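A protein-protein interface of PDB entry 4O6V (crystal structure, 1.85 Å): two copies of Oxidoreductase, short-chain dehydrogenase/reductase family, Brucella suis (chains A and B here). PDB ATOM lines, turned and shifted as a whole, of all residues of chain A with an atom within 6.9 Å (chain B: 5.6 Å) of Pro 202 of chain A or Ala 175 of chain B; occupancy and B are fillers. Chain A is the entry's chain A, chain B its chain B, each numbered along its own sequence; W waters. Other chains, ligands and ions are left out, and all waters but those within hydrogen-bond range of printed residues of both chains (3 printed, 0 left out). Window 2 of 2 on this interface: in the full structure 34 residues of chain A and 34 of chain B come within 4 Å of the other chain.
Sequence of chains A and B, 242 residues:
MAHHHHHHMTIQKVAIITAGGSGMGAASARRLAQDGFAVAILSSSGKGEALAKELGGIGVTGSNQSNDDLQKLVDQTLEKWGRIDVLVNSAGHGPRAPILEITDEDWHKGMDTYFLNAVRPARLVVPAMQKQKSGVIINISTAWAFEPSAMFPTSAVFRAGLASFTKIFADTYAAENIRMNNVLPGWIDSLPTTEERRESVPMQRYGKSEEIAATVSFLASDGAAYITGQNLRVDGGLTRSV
OD2 of Asp 171 of chain B lies within salt-bridge range of NH1 of Arg 240 of chain A (2.9 Å).
O of Pro 202 of chain A is in hydrogen-bond range of N of Ala 175 of chain B, 3.4 Å away.
The backbone carbonyl oxygen of Gly 237 of chain A is in hydrogen-bond range of the guanidinium group of Arg 240 of chain A (2.7 Å).
OD1 of Asp 235 of chain A sits close to N of Gly 237 of chain A.
The backbone carbonyl oxygen (O) of Gly 236 of chain A is in hydrogen-bond range of the backbone NH (N) of Met 203 of chain A (3.1 Å).
The guanidinium group (NE) of Arg 240 of chain A sits at hydrogen-bond distance from the backbone carbonyl oxygen (O) of Leu 238 of chain A (3.1 Å).
Among the printed residues, pairs that only touch across the chains: Pro 202 of chain A with Asp 171 of chain B, Pro 202 of chain A with Ala 174 of chain B, Met 203 of chain A with Ala 174 of chain B, Met 203 of chain A with Asn 177 of chain B and Gly 237 of chain A with Asp 171 of chain B.
Of the printed residues of chain B, Arg 240 of chain A touches Asp 171.
Ala 170 of chain B touches none of the printed residues of chain A.
Printed residues of chain A within 4 Å of Ala 174 of chain B: Pro 202 (3.4 Å) and Met 203 (3.5 Å).
Glu 176 of chain B touches none of the printed residues of chain A.
Hydrophobic or aromatic side chains of chain B that line the printed part of chain A: Ala 174.
Printed residues of chain A that touch a printed residue of chain B: Pro 202, Met 203, Gly 237 and Arg 240.
Hydrophobic or aromatic side chains of chain A that line the printed part of chain B: Pro 202 and Met 203.
Among the printed residues, 7 pairs touch across the chains.
Among the printed residues, Asp or Glu carboxylates within 4 Å of a Lys or Arg side-chain nitrogen of the other chain: Arg 240 of chain A with Asp 171 of chain B (2.9 Å).
No position is printed for both chains.
Of the 7 pairs that touch across the chains among the printed residues, none has its exchanged pair printed and touching as well.
Water W3 lies within hydrogen-bond range of O of Ala 174 of chain B and O of Met 203 of chain A.
Water W1 bridges OD1 of Asn 177 of chain B and NH2 of Arg 205 of chain A.
Water W2 bridges OD1 of Asn 177 of chain B and NE of Arg 205 of chain A.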
ATOM      1  N   ARG A 198     -14.974  27.895  31.108  1.00  0.00           N
ATOM      2  CA  ARG A 198     -15.288  27.973  29.696  1.00  0.00           C
ATOM      3  C   ARG A 198     -16.457  27.075  29.300  1.00  0.00           C
ATOM      4  O   ARG A 198     -17.357  27.495  28.563  1.00  0.00           O
ATOM      5  CB  ARG A 198     -14.069  27.636  28.854  1.00  0.00           C
ATOM      6  CG  ARG A 198     -14.286  27.971  27.384  1.00  0.00           C
ATOM      7  CD  ARG A 198     -13.207  27.435  26.475  1.00  0.00           C
ATOM      8  NE  ARG A 198     -12.942  26.005  26.628  1.00  0.00           N
ATOM      9  CZ  ARG A 198     -13.649  25.014  26.089  1.00  0.00           C
ATOM     10  NH1 ARG A 198     -14.741  25.241  25.351  1.00  0.00           N
ATOM     11  NH2 ARG A 198     -13.238  23.752  26.280  1.00  0.00           N
ATOM     12  N   GLU A 199     -16.451  25.842  29.800  1.00  0.00           N
ATOM     13  CA  GLU A 199     -17.549  24.901  29.546  1.00  0.00           C
ATOM     14  C   GLU A 199     -18.901  25.233  30.170  1.00  0.00           C
ATOM     15  O   GLU A 199     -19.933  24.752  29.688  1.00  0.00           O
ATOM     16  CB  GLU A 199     -17.100  23.464  29.908  1.00  0.00           C
ATOM     17  CG  GLU A 199     -16.107  22.942  28.894  1.00  0.00           C
ATOM     18  CD  GLU A 199     -15.819  21.458  29.066  1.00  0.00           C
ATOM     19  OE1 GLU A 199     -16.423  20.830  29.952  1.00  0.00           O
ATOM     20  OE2 GLU A 199     -14.954  20.940  28.335  1.00  0.00           O
ATOM     21  N   SER A 200     -18.910  26.080  31.201  1.00  0.00           N
ATOM     22  CA  SER A 200     -20.158  26.510  31.879  1.00  0.00           C
ATOM     23  C   SER A 200     -20.949  27.528  31.050  1.00  0.00           C
ATOM     24  O   SER A 200     -22.133  27.757  31.253  1.00  0.00           O
ATOM     25  CB  SER A 200     -19.834  27.098  33.251  1.00  0.00           C
ATOM     26  OG  SER A 200     -19.229  28.409  33.207  1.00  0.00           O
ATOM     27  N   VAL A 201     -20.253  28.150  30.117  1.00  0.00           N
ATOM     28  CA  VAL A 201     -20.848  29.103  29.212  1.00  0.00           C
ATOM     29  C   VAL A 201     -21.512  28.356  28.041  1.00  0.00           C
ATOM     30  O   VAL A 201     -20.843  27.608  27.322  1.00  0.00           O
ATOM     31  CB  VAL A 201     -19.771  30.056  28.611  1.00  0.00           C
ATOM     32  CG1 VAL A 201     -20.447  31.123  27.759  1.00  0.00           C
ATOM     33  CG2 VAL A 201     -18.966  30.736  29.701  1.00  0.00           C
ATOM     34  N   PRO A 202     -22.817  28.580  27.791  1.00  0.00           N
ATOM     35  CA  PRO A 202     -23.413  27.844  26.649  1.00  0.00           C
ATOM     36  C   PRO A 202     -22.712  28.034  25.328  1.00  0.00           C
ATOM     37  O   PRO A 202     -22.640  27.087  24.557  1.00  0.00           O
ATOM     38  CB  PRO A 202     -24.827  28.405  26.574  1.00  0.00           C
ATOM     39  CG  PRO A 202     -25.130  28.656  28.017  1.00  0.00           C
ATOM     40  CD  PRO A 202     -23.871  29.228  28.601  1.00  0.00           C
ATOM     41  N   MET A 203     -22.229  29.243  25.065  1.00  0.00           N
ATOM     42  CA  MET A 203     -21.430  29.506  23.851  1.00  0.00           C
ATOM     43  C   MET A 203     -20.058  28.827  23.828  1.00  0.00           C
ATOM     44  O   MET A 203     -19.435  28.823  22.789  1.00  0.00           O
ATOM     45  CB  MET A 203     -21.294  31.013  23.592  1.00  0.00           C
ATOM     46  CG  MET A 203     -22.613  31.571  23.110  1.00  0.00           C
ATOM     47  SD  MET A 203     -22.596  33.304  22.531  1.00  0.00           S
ATOM     48  CE  MET A 203     -21.577  33.221  21.124  1.00  0.00           C
ATOM     49  N   GLN A 204     -19.610  28.269  24.951  1.00  0.00           N
ATOM     50  CA  GLN A 204     -18.396  27.399  25.017  1.00  0.00           C
ATOM     51  C   GLN A 204     -17.085  28.193  24.787  1.00  0.00           C
ATOM     52  O   GLN A 204     -16.081  27.647  24.375  1.00  0.00           O
ATOM     53  CB  GLN A 204     -18.492  26.190  24.075  1.00  0.00           C
ATOM     54  CG  GLN A 204     -19.650  25.239  24.413  1.00  0.00           C
ATOM     55  CD  GLN A 204     -19.445  24.555  25.755  1.00  0.00           C
ATOM     56  OE1 GLN A 204     -18.599  23.685  25.868  1.00  0.00           O
ATOM     57  NE2 GLN A 204     -20.246  24.912  26.755  1.00  0.00           N
ATOM     58  N   ARG A 205     -17.130  29.480  25.069  1.00  0.00           N
ATOM     59  CA  ARG A 205     -15.985  30.390  24.932  1.00  0.00           C
ATOM     60  C   ARG A 205     -16.159  31.562  25.879  1.00  0.00           C
ATOM     61  O   ARG A 205     -17.288  31.941  26.259  1.00  0.00           O
ATOM     62  CB  ARG A 205     -15.884  30.940  23.510  1.00  0.00           C
ATOM     63  CG  ARG A 205     -16.996  31.924  23.097  1.00  0.00           C
ATOM     64  CD  ARG A 205     -16.644  32.515  21.742  1.00  0.00           C
ATOM     65  NE  ARG A 205     -17.628  33.408  21.168  1.00  0.00           N
ATOM     66  CZ  ARG A 205     -17.670  34.714  21.359  1.00  0.00           C
ATOM     67  NH1 ARG A 205     -16.798  35.312  22.175  1.00  0.00           N
ATOM     68  NH2 ARG A 205     -18.576  35.444  20.704  1.00  0.00           N
ATOM     69  N   ASP A 235     -22.760  37.734  28.216  1.00  0.00           N
ATOM     70  CA  ASP A 235     -22.178  36.596  28.956  1.00  0.00           C
ATOM     71  C   ASP A 235     -22.271  35.231  28.256  1.00  0.00           C
ATOM     72  O   ASP A 235     -22.107  34.178  28.899  1.00  0.00           O
ATOM     73  CB  ASP A 235     -22.822  36.560  30.349  1.00  0.00           C
ATOM     74  CG  ASP A 235     -24.317  36.110  30.330  1.00  0.00           C
ATOM     75  OD1 ASP A 235     -24.921  35.963  29.219  1.00  0.00           O
ATOM     76  OD2 ASP A 235     -24.825  35.848  31.451  1.00  0.00           O
ATOM     77  N   GLY A 236     -22.533  35.219  26.937  1.00  0.00           N
ATOM     78  CA  GLY A 236     -22.551  33.948  26.221  1.00  0.00           C
ATOM     79  C   GLY A 236     -23.623  32.986  26.654  1.00  0.00           C
ATOM     80  O   GLY A 236     -23.559  31.767  26.345  1.00  0.00           O
ATOM     81  N   GLY A 237     -24.598  33.505  27.408  1.00  0.00           N
ATOM     82  CA  GLY A 237     -25.715  32.716  27.882  1.00  0.00           C
ATOM     83  C   GLY A 237     -25.501  32.160  29.255  1.00  0.00           C
ATOM     84  O   GLY A 237     -26.258  31.321  29.694  1.00  0.00           O
ATOM     85  N   LEU A 238     -24.471  32.617  29.945  1.00  0.00           N
ATOM     86  CA  LEU A 238     -24.074  32.009  31.206  1.00  0.00           C
ATOM     87  C   LEU A 238     -25.183  31.983  32.249  1.00  0.00           C
ATOM     88  O   LEU A 238     -25.501  30.927  32.844  1.00  0.00           O
ATOM     89  CB  LEU A 238     -22.840  32.737  31.787  1.00  0.00           C
ATOM     90  CG  LEU A 238     -22.276  32.279  33.164  1.00  0.00           C
ATOM     91  CD1 LEU A 238     -21.817  30.837  33.168  1.00  0.00           C
ATOM     92  CD2 LEU A 238     -21.130  33.191  33.596  1.00  0.00           C
ATOM     93  N   THR A 239     -25.698  33.158  32.552  1.00  0.00           N
ATOM     94  CA  THR A 239     -26.696  33.334  33.592  1.00  0.00           C
ATOM     95  C   THR A 239     -28.013  32.715  33.118  1.00  0.00           C
ATOM     96  O   THR A 239     -28.275  32.537  31.874  1.00  0.00           O
ATOM     97  CB  THR A 239     -26.915  34.832  33.893  1.00  0.00           C
ATOM     98  OG1 THR A 239     -27.098  35.528  32.649  1.00  0.00           O
ATOM     99  CG2 THR A 239     -25.743  35.408  34.609  1.00  0.00           C
ATOM    100  N   ARG A 240     -28.830  32.366  34.106  1.00  0.00           N
ATOM    101  CA  ARG A 240     -30.008  31.564  33.886  1.00  0.00           C
ATOM    102  C   ARG A 240     -31.303  32.316  33.702  1.00  0.00           C
ATOM    103  O   ARG A 240     -32.234  31.788  33.098  1.00  0.00           O
ATOM    104  CB  ARG A 240     -30.222  30.587  35.070  1.00  0.00           C
ATOM    105  CG  ARG A 240     -29.051  29.706  35.422  1.00  0.00           C
ATOM    106  CD  ARG A 240     -28.674  28.656  34.386  1.00  0.00           C
ATOM    107  NE  ARG A 240     -28.026  29.175  33.176  1.00  0.00           N
ATOM    108  CZ  ARG A 240     -28.384  28.846  31.927  1.00  0.00           C
ATOM    109  NH1 ARG A 240     -29.370  27.977  31.713  1.00  0.00           N
ATOM    110  NH2 ARG A 240     -27.727  29.335  30.878  1.00  0.00           N
ATOM    111  N   ALA B 170     -31.726  29.820  23.261  1.00  0.00           N
ATOM    112  CA  ALA B 170     -30.398  30.339  23.355  1.00  0.00           C
ATOM    113  C   ALA B 170     -29.473  29.292  23.969  1.00  0.00           C
ATOM    114  O   ALA B 170     -28.341  29.145  23.523  1.00  0.00           O
ATOM    115  CB  ALA B 170     -30.400  31.591  24.200  1.00  0.00           C
ATOM    116  N   ASP B 171     -29.961  28.586  24.990  1.00  0.00           N
ATOM    117  CA  ASP B 171     -29.150  27.551  25.608  1.00  0.00           C
ATOM    118  C   ASP B 171     -28.957  26.348  24.647  1.00  0.00           C
ATOM    119  O   ASP B 171     -27.914  25.728  24.639  1.00  0.00           O
ATOM    120  CB  ASP B 171     -29.771  27.075  26.897  1.00  0.00           C
ATOM    121  CG  ASP B 171     -29.566  28.062  28.064  1.00  0.00           C
ATOM    122  OD1 ASP B 171     -28.671  28.901  28.018  1.00  0.00           O
ATOM    123  OD2 ASP B 171     -30.340  28.019  29.029  1.00  0.00           O
ATOM    124  N   THR B 172     -29.981  26.033  23.853  1.00  0.00           N
ATOM    125  CA  THR B 172     -29.951  24.869  22.964  1.00  0.00           C
ATOM    126  C   THR B 172     -28.981  25.077  21.812  1.00  0.00           C
ATOM    127  O   THR B 172     -28.303  24.133  21.431  1.00  0.00           O
ATOM    128  CB  THR B 172     -31.365  24.549  22.462  1.00  0.00           C
ATOM    129  OG1 THR B 172     -32.193  24.292  23.626  1.00  0.00           O
ATOM    130  CG2 THR B 172     -31.366  23.356  21.501  1.00  0.00           C
ATOM    131  N   TYR B 173     -28.926  26.301  21.261  1.00  0.00           N
ATOM    132  CA  TYR B 173     -28.150  26.589  20.067  1.00  0.00           C
ATOM    133  C   TYR B 173     -26.884  27.425  20.252  1.00  0.00           C
ATOM    134  O   TYR B 173     -26.195  27.675  19.293  1.00  0.00           O
ATOM    135  CB  TYR B 173     -29.061  27.192  18.986  1.00  0.00           C
ATOM    136  CG  TYR B 173     -30.111  26.199  18.527  1.00  0.00           C
ATOM    137  CD1 TYR B 173     -29.792  25.188  17.646  1.00  0.00           C
ATOM    138  CD2 TYR B 173     -31.425  26.254  19.017  1.00  0.00           C
ATOM    139  CE1 TYR B 173     -30.741  24.264  17.225  1.00  0.00           C
ATOM    140  CE2 TYR B 173     -32.376  25.309  18.615  1.00  0.00           C
ATOM    141  CZ  TYR B 173     -32.040  24.327  17.735  1.00  0.00           C
ATOM    142  OH  TYR B 173     -33.004  23.420  17.367  1.00  0.00           O
ATOM    143  N   ALA B 174     -26.546  27.810  21.477  1.00  0.00           N
ATOM    144  CA  ALA B 174     -25.361  28.622  21.726  1.00  0.00           C
ATOM    145  C   ALA B 174     -24.066  27.987  21.213  1.00  0.00           C
ATOM    146  O   ALA B 174     -23.204  28.677  20.697  1.00  0.00           O
ATOM    147  CB  ALA B 174     -25.218  28.875  23.221  1.00  0.00           C
ATOM    148  N   ALA B 175     -23.929  26.683  21.420  1.00  0.00           N
ATOM    149  CA  ALA B 175     -22.735  25.939  20.980  1.00  0.00           C
ATOM    150  C   ALA B 175     -22.502  25.987  19.461  1.00  0.00           C
ATOM    151  O   ALA B 175     -21.385  25.887  19.028  1.00  0.00           O
ATOM    152  CB  ALA B 175     -22.818  24.488  21.439  1.00  0.00           C
ATOM    153  N   GLU B 176     -23.561  26.224  18.691  1.00  0.00           N
ATOM    154  CA  GLU B 176     -23.526  26.346  17.235  1.00  0.00           C
ATOM    155  C   GLU B 176     -23.471  27.838  16.782  1.00  0.00           C
ATOM    156  O   GLU B 176     -23.597  28.138  15.613  1.00  0.00           O
ATOM    157  CB  GLU B 176     -24.760  25.637  16.654  1.00  0.00           C
ATOM    158  CG  GLU B 176     -24.743  24.115  16.778  1.00  0.00           C
ATOM    159  CD  GLU B 176     -25.965  23.466  16.115  1.00  0.00           C
ATOM    160  OE1 GLU B 176     -27.030  23.380  16.746  1.00  0.00           O
ATOM    161  OE2 GLU B 176     -25.890  23.108  14.947  1.00  0.00           O
ATOM    162  N   ASN B 177     -23.232  28.744  17.731  1.00  0.00           N
ATOM    163  CA  ASN B 177     -23.070  30.171  17.463  1.00  0.00           C
ATOM    164  C   ASN B 177     -24.321  30.826  16.878  1.00  0.00           C
ATOM    165  O   ASN B 177     -24.235  31.770  16.082  1.00  0.00           O
ATOM    166  CB  ASN B 177     -21.889  30.392  16.548  1.00  0.00           C
ATOM    167  CG  ASN B 177     -21.422  31.794  16.541  1.00  0.00           C
ATOM    168  OD1 ASN B 177     -21.464  32.462  17.550  1.00  0.00           O
ATOM    169  ND2 ASN B 177     -21.031  32.277  15.378  1.00  0.00           N
HETATM  170  O   HOH W   1     -19.706  34.494  18.256  1.00  0.00           O
HETATM  171  O   HOH W   2     -19.320  31.656  19.424  1.00  0.00           O
HETATM  172  O   HOH W   3     -20.608  29.254  20.252  1.00  0.00           O
